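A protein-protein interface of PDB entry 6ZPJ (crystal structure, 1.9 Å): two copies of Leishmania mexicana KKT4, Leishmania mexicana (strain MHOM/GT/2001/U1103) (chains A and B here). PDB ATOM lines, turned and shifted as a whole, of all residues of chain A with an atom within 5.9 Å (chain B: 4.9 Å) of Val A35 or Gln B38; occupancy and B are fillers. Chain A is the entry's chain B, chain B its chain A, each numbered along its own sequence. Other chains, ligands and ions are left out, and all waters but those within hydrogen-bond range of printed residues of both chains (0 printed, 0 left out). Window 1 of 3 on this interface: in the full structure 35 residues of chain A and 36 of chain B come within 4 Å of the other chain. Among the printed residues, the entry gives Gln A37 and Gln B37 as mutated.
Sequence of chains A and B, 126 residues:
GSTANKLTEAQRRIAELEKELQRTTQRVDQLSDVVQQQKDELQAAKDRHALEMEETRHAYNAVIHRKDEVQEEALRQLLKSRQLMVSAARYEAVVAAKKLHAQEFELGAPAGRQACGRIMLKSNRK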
ATOM      1  N   GLN A  30       9.421 -16.426  15.485  1.00  0.00           N
ATOM      2  CA  GLN A  30       8.293 -15.892  16.258  1.00  0.00           C
ATOM      3  C   GLN A  30       8.629 -14.527  16.837  1.00  0.00           C
ATOM      4  O   GLN A  30       7.844 -13.589  16.744  1.00  0.00           O
ATOM      5  CB  GLN A  30       7.905 -16.875  17.383  1.00  0.00           C
ATOM      6  CG  GLN A  30       7.057 -18.073  16.914  1.00  0.00           C
ATOM      7  CD  GLN A  30       5.559 -17.814  16.913  1.00  0.00           C
ATOM      8  OE1 GLN A  30       5.099 -16.788  17.416  1.00  0.00           O
ATOM      9  NE2 GLN A  30       4.778 -18.757  16.338  1.00  0.00           N
ATOM     10  N   LEU A  31       9.802 -14.395  17.428  1.00  0.00           N
ATOM     11  CA  LEU A  31      10.219 -13.108  17.966  1.00  0.00           C
ATOM     12  C   LEU A  31      10.402 -12.061  16.867  1.00  0.00           C
ATOM     13  O   LEU A  31      10.103 -10.889  17.099  1.00  0.00           O
ATOM     14  CB  LEU A  31      11.518 -13.326  18.731  1.00  0.00           C
ATOM     15  CG  LEU A  31      11.318 -13.973  20.099  1.00  0.00           C
ATOM     16  CD1 LEU A  31      12.729 -14.320  20.696  1.00  0.00           C
ATOM     17  CD2 LEU A  31      10.547 -13.039  21.032  1.00  0.00           C
ATOM     18  N   SER A  32      10.924 -12.454  15.683  1.00  0.00           N
ATOM     19  CA  SER A  32      11.045 -11.510  14.563  1.00  0.00           C
ATOM     20  C   SER A  32       9.688 -10.970  14.160  1.00  0.00           C
ATOM     21  O   SER A  32       9.554  -9.788  13.799  1.00  0.00           O
ATOM     22  CB  SER A  32      11.721 -12.163  13.354  1.00  0.00           C
ATOM     23  OG  SER A  32      13.052 -12.514  13.705  1.00  0.00           O
ATOM     24  N   ASP A  33       8.669 -11.835  14.193  1.00  0.00           N
ATOM     25  CA  ASP A  33       7.311 -11.387  13.914  1.00  0.00           C
ATOM     26  C   ASP A  33       6.830 -10.368  14.950  1.00  0.00           C
ATOM     27  O   ASP A  33       6.239  -9.353  14.573  1.00  0.00           O
ATOM     28  CB  ASP A  33       6.338 -12.569  13.838  1.00  0.00           C
ATOM     29  CG  ASP A  33       4.972 -12.141  13.294  1.00  0.00           C
ATOM     30  OD1 ASP A  33       4.897 -11.791  12.098  1.00  0.00           O
ATOM     31  OD2 ASP A  33       3.988 -12.120  14.072  1.00  0.00           O
ATOM     32  N   VAL A  34       7.083 -10.610  16.245  1.00  0.00           N
ATOM     33  CA  VAL A  34       6.684  -9.655  17.285  1.00  0.00           C
ATOM     34  C   VAL A  34       7.380  -8.325  17.047  1.00  0.00           C
ATOM     35  O   VAL A  34       6.794  -7.247  17.213  1.00  0.00           O
ATOM     36  CB  VAL A  34       7.033 -10.207  18.680  1.00  0.00           C
ATOM     37  CG1 VAL A  34       6.777  -9.127  19.771  1.00  0.00           C
ATOM     38  CG2 VAL A  34       6.223 -11.473  19.001  1.00  0.00           C
ATOM     39  N   VAL A  35       8.653  -8.386  16.664  1.00  0.00           N
ATOM     40  CA  VAL A  35       9.418  -7.152  16.511  1.00  0.00           C
ATOM     41  C   VAL A  35       8.811  -6.318  15.408  1.00  0.00           C
ATOM     42  O   VAL A  35       8.665  -5.095  15.535  1.00  0.00           O
ATOM     43  CB  VAL A  35      10.901  -7.447  16.225  1.00  0.00           C
ATOM     44  CG1 VAL A  35      11.572  -6.139  15.755  1.00  0.00           C
ATOM     45  CG2 VAL A  35      11.562  -7.916  17.538  1.00  0.00           C
ATOM     46  N   GLN A  36       8.447  -6.966  14.304  1.00  0.00           N
ATOM     47  CA  GLN A  36       7.851  -6.195  13.232  1.00  0.00           C
ATOM     48  C   GLN A  36       6.469  -5.691  13.610  1.00  0.00           C
ATOM     49  O   GLN A  36       6.082  -4.586  13.212  1.00  0.00           O
ATOM     50  CB  GLN A  36       7.787  -7.023  11.962  1.00  0.00           C
ATOM     51  CG  GLN A  36       7.309  -6.143  10.762  1.00  0.00           C
ATOM     52  CD  GLN A  36       8.342  -5.083  10.367  1.00  0.00           C
ATOM     53  OE1 GLN A  36       9.481  -5.401  10.020  1.00  0.00           O
ATOM     54  NE2 GLN A  36       7.942  -3.824  10.430  1.00  0.00           N
ATOM     55  N   GLN A  37       5.690  -6.502  14.329  1.00  0.00           N
ATOM     56  CA  GLN A  37       4.368  -6.052  14.720  1.00  0.00           C
ATOM     57  C   GLN A  37       4.465  -4.838  15.623  1.00  0.00           C
ATOM     58  O   GLN A  37       3.682  -3.907  15.490  1.00  0.00           O
ATOM     59  CB  GLN A  37       3.599  -7.171  15.408  1.00  0.00           C
ATOM     60  CG  GLN A  37       3.102  -8.228  14.425  1.00  0.00           C
ATOM     61  CD  GLN A  37       1.972  -9.038  14.993  1.00  0.00           C
ATOM     62  OE1 GLN A  37       1.296  -8.607  15.933  1.00  0.00           O
ATOM     63  NE2 GLN A  37       1.738 -10.211  14.416  1.00  0.00           N
ATOM     64  N   GLN A  38       5.433  -4.832  16.540  1.00  0.00           N
ATOM     65  CA  GLN A  38       5.637  -3.677  17.393  1.00  0.00           C
ATOM     66  C   GLN A  38       6.031  -2.444  16.601  1.00  0.00           C
ATOM     67  O   GLN A  38       5.608  -1.343  16.942  1.00  0.00           O
ATOM     68  CB  GLN A  38       6.717  -3.983  18.423  1.00  0.00           C
ATOM     69  CG  GLN A  38       6.303  -4.947  19.493  1.00  0.00           C
ATOM     70  CD  GLN A  38       7.494  -5.213  20.435  1.00  0.00           C
ATOM     71  OE1 GLN A  38       8.651  -5.345  19.973  1.00  0.00           O
ATOM     72  NE2 GLN A  38       7.243  -5.203  21.713  1.00  0.00           N
ATOM     73  N   LYS A  39       6.933  -2.591  15.623  1.00  0.00           N
ATOM     74  CA  LYS A  39       7.319  -1.467  14.769  1.00  0.00           C
ATOM     75  C   LYS A  39       6.123  -0.890  14.035  1.00  0.00           C
ATOM     76  O   LYS A  39       5.962   0.340  13.970  1.00  0.00           O
ATOM     77  CB  LYS A  39       8.370  -1.902  13.753  1.00  0.00           C
ATOM     78  CG  LYS A  39       9.745  -2.035  14.336  1.00  0.00           C
ATOM     79  CD  LYS A  39      10.738  -2.513  13.262  1.00  0.00           C
ATOM     80  CE  LYS A  39      12.110  -2.736  13.898  1.00  0.00           C
ATOM     81  NZ  LYS A  39      13.066  -3.193  12.847  1.00  0.00           N
ATOM     82  N   ASP A  40       5.266  -1.773  13.479  1.00  0.00           N
ATOM     83  CA  ASP A  40       4.048  -1.333  12.809  1.00  0.00           C
ATOM     84  C   ASP A  40       3.125  -0.601  13.764  1.00  0.00           C
ATOM     85  O   ASP A  40       2.532   0.413  13.388  1.00  0.00           O
ATOM     86  CB  ASP A  40       3.303  -2.521  12.191  1.00  0.00           C
ATOM     87  CG  ASP A  40       4.086  -3.206  11.087  1.00  0.00           C
ATOM     88  OD1 ASP A  40       5.087  -2.627  10.589  1.00  0.00           O
ATOM     89  OD2 ASP A  40       3.706  -4.358  10.744  1.00  0.00           O
ATOM     90  N   LEU B  31      16.836 -10.465  19.982  1.00  0.00           N
ATOM     91  CA  LEU B  31      15.458 -10.122  19.639  1.00  0.00           C
ATOM     92  C   LEU B  31      14.621  -9.925  20.891  1.00  0.00           C
ATOM     93  O   LEU B  31      13.739  -9.062  20.919  1.00  0.00           O
ATOM     94  CB  LEU B  31      14.809 -11.206  18.752  1.00  0.00           C
ATOM     95  CG  LEU B  31      15.465 -11.274  17.352  1.00  0.00           C
ATOM     96  CD1 LEU B  31      15.130 -12.547  16.632  1.00  0.00           C
ATOM     97  CD2 LEU B  31      14.974 -10.069  16.510  1.00  0.00           C
ATOM     98  N   VAL B  34      15.104  -6.498  22.058  1.00  0.00           N
ATOM     99  CA  VAL B  34      14.393  -5.538  21.220  1.00  0.00           C
ATOM    100  C   VAL B  34      12.912  -5.504  21.572  1.00  0.00           C
ATOM    101  O   VAL B  34      12.307  -4.428  21.646  1.00  0.00           O
ATOM    102  CB  VAL B  34      14.609  -5.845  19.732  1.00  0.00           C
ATOM    103  CG1 VAL B  34      13.796  -4.874  18.890  1.00  0.00           C
ATOM    104  CG2 VAL B  34      16.093  -5.736  19.388  1.00  0.00           C
ATOM    105  N   VAL B  35      12.313  -6.677  21.822  1.00  0.00           N
ATOM    106  CA  VAL B  35      10.885  -6.736  22.123  1.00  0.00           C
ATOM    107  C   VAL B  35      10.589  -5.935  23.378  1.00  0.00           C
ATOM    108  O   VAL B  35       9.658  -5.136  23.404  1.00  0.00           O
ATOM    109  CB  VAL B  35      10.412  -8.197  22.264  1.00  0.00           C
ATOM    110  CG1 VAL B  35       8.984  -8.221  22.759  1.00  0.00           C
ATOM    111  CG2 VAL B  35      10.449  -8.835  20.892  1.00  0.00           C
ATOM    112  N   GLN B  36      11.384  -6.134  24.433  1.00  0.00           N
ATOM    113  CA  GLN B  36      11.143  -5.413  25.688  1.00  0.00           C
ATOM    114  C   GLN B  36      11.394  -3.917  25.536  1.00  0.00           C
ATOM    115  O   GLN B  36      10.611  -3.100  26.045  1.00  0.00           O
ATOM    116  CB  GLN B  36      11.997  -5.994  26.820  1.00  0.00           C
ATOM    117  CG  GLN B  36      11.552  -7.396  27.323  1.00  0.00           C
ATOM    118  CD  GLN B  36      10.029  -7.575  27.564  1.00  0.00           C
ATOM    119  OE1 GLN B  36       9.372  -8.353  26.859  1.00  0.00           O
ATOM    120  NE2 GLN B  36       9.480  -6.898  28.590  1.00  0.00           N
ATOM    121  N   GLN B  37      12.455  -3.528  24.823  1.00  0.00           N
ATOM    122  CA  GLN B  37      12.683  -2.101  24.596  1.00  0.00           C
ATOM    123  C   GLN B  37      11.544  -1.454  23.801  1.00  0.00           C
ATOM    124  O   GLN B  37      11.159  -0.307  24.080  1.00  0.00           O
ATOM    125  CB  GLN B  37      14.000  -1.878  23.862  1.00  0.00           C
ATOM    126  CG  GLN B  37      15.249  -2.274  24.623  1.00  0.00           C
ATOM    127  CD  GLN B  37      16.455  -2.517  23.685  1.00  0.00           C
ATOM    128  OE1 GLN B  37      16.314  -2.518  22.458  1.00  0.00           O
ATOM    129  NE2 GLN B  37      17.637  -2.730  24.267  1.00  0.00           N
ATOM    130  N   GLN B  38      10.998  -2.164  22.797  1.00  0.00           N
ATOM    131  CA  GLN B  38       9.924  -1.605  22.005  1.00  0.00           C
ATOM    132  C   GLN B  38       8.639  -1.489  22.799  1.00  0.00           C
ATOM    133  O   GLN B  38       7.860  -0.572  22.543  1.00  0.00           O
ATOM    134  CB  GLN B  38       9.698  -2.423  20.733  1.00  0.00           C
ATOM    135  CG  GLN B  38      10.927  -2.285  19.799  1.00  0.00           C
ATOM    136  CD  GLN B  38      10.779  -2.780  18.390  1.00  0.00           C
ATOM    137  OE1 GLN B  38      11.462  -2.284  17.481  1.00  0.00           O
ATOM    138  NE2 GLN B  38       9.937  -3.775  18.190  1.00  0.00           N
ATOM    139  N   LYS B  39       8.386  -2.413  23.730  1.00  0.00           N
ATOM    140  CA  LYS B  39       7.260  -2.258  24.653  1.00  0.00           C
ATOM    141  C   LYS B  39       7.356  -0.950  25.425  1.00  0.00           C
ATOM    142  O   LYS B  39       6.372  -0.195  25.534  1.00  0.00           O
ATOM    143  CB  LYS B  39       7.208  -3.434  25.641  1.00  0.00           C
ATOM    144  CG  LYS B  39       6.633  -4.696  25.093  1.00  0.00           C
ATOM    145  CD  LYS B  39       6.735  -5.822  26.157  1.00  0.00           C
ATOM    146  CE  LYS B  39       6.151  -7.143  25.652  1.00  0.00           C
ATOM    147  NZ  LYS B  39       6.570  -8.323  26.494  1.00  0.00           N
ATOM    148  N   ASP B  40       8.526  -0.704  26.028  1.00  0.00           N
ATOM    149  CA  ASP B  40       8.778   0.532  26.767  1.00  0.00           C
ATOM    150  C   ASP B  40       8.619   1.750  25.875  1.00  0.00           C
ATOM    151  O   ASP B  40       7.978   2.741  26.258  1.00  0.00           O
ATOM    152  CB  ASP B  40      10.185   0.502  27.357  1.00  0.00           C
ATOM    153  CG  ASP B  40      10.342  -0.543  28.470  1.00  0.00           C
ATOM    154  OD1 ASP B  40       9.323  -1.111  28.937  1.00  0.00           O
ATOM    155  OD2 ASP B  40      11.501  -0.816  28.867  1.00  0.00           O
ATOM    156  N   GLU B  41       9.220   1.704  24.688  1.00  0.00           N
ATOM    157  CA  GLU B  41       9.082   2.792  23.717  1.00  0.00           C
ATOM    158  C   GLU B  41       7.618   3.079  23.382  1.00  0.00           C
ATOM    159  O   GLU B  41       7.196   4.247  23.326  1.00  0.00           O
ATOM    160  CB  GLU B  41       9.879   2.429  22.459  1.00  0.00           C
ATOM    161  CG  GLU B  41       9.897   3.477  21.357  1.00  0.00           C
ATOM    162  CD  GLU B  41      10.690   3.032  20.093  1.00  0.00           C
ATOM    163  OE1 GLU B  41      10.992   1.821  19.938  1.00  0.00           O
ATOM    164  OE2 GLU B  41      11.010   3.903  19.240  1.00  0.00           O
ATOM    165  N   LEU B  42       6.832   2.030  23.106  1.00  0.00           N
ATOM    166  CA  LEU B  42       5.431   2.227  22.750  1.00  0.00           C
ATOM    167  C   LEU B  42       4.692   2.986  23.837  1.00  0.00           C
ATOM    168  O   LEU B  42       3.951   3.938  23.559  1.00  0.00           O
ATOM    169  CB  LEU B  42       4.748   0.880  22.510  1.00  0.00           C
ATOM    170  CG  LEU B  42       3.279   1.108  22.148  1.00  0.00           C
ATOM    171  CD1 LEU B  42       3.132   1.954  20.872  1.00  0.00           C
ATOM    172  CD2 LEU B  42       2.504  -0.212  22.033  1.00  0.00           C
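NE2 of Gln A38 is in hydrogen-bond range of O of Val B35 (2.9 Å). The side-chain amide nitrogen (NE2) of Gln B38 is in hydrogen-bond range of the backbone carbonyl oxygen (O) of Val A35. The side-chain amide oxygen (OE1) of Gln A38 is in hydrogen-bond range of the side-chain amide nitrogen (NE2) of Gln B38.
The side-chain amide oxygen of Gln B36 is in hydrogen-bond range of the side-chain amino group of Lys B39, at 2.8 Å.
Leu A31 touches Leu B31 (CB to CB, 3.9 Å). OG of Ser A32 touches CD1 of Leu B31, 3.6 Å away. CG1 of Val A34 touches CG1 of Val B35, at 3.8 Å. Val A35 touches Val B35 (CG2 to CG2, 3.7 Å). NE2 of Gln A38 touches CG of Lys B39, 3.5 Å away. Lys A39 touches Gln B38 (CG to OE1, 3.6 Å).
Of chain A, only Val A35, Gln A38 and Lys A39 come within 4 Å of Gln B38. Of the printed residues of chain B, Gln A38 touches Val B35, Gln B38 and Lys B39. Of the printed residues of chain B, Ser A32 touches Leu B31. Printed residues of chain A within 4 Å of Leu B31: Leu A31 (3.9 Å) and Ser A32 (3.6 Å). Printed residues of chain B within 4 Å of Val A34: Val B35. Of the printed residues of chain A, Val B35 touches Val A34, Val A35 and Gln A38. Leu B42 touches none of the printed residues of chain A. The nearest printed residue of chain B that does not touch Ser A32 is Val B35 (6.4 Å).
Of the 10 printed residues of chain B, 4 touch a printed residue of chain A. Printed residues of chain B that touch a printed residue of chain A: Leu B31, Val B35, Gln B38 and Lys B39. Of the 11 printed residues of chain A, 6 touch a printed residue of chain B. Printed residues of chain A that touch a printed residue of chain B: Leu A31, Ser A32, Val A34, Val A35, Gln A38 and Lys A39.
Leu B31 touches its own counterpart, Leu A31. Val A34 touches Val B35, but with the chains exchanged Val A35 does not touch Val B34 (4.01 Å). Val A35 touches its own counterpart, Val B35. Gln A38 touches its own counterpart, Gln B38. Positions printed for both chains: 31, 34, 35, 36, 37, 38, 39 and 40.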
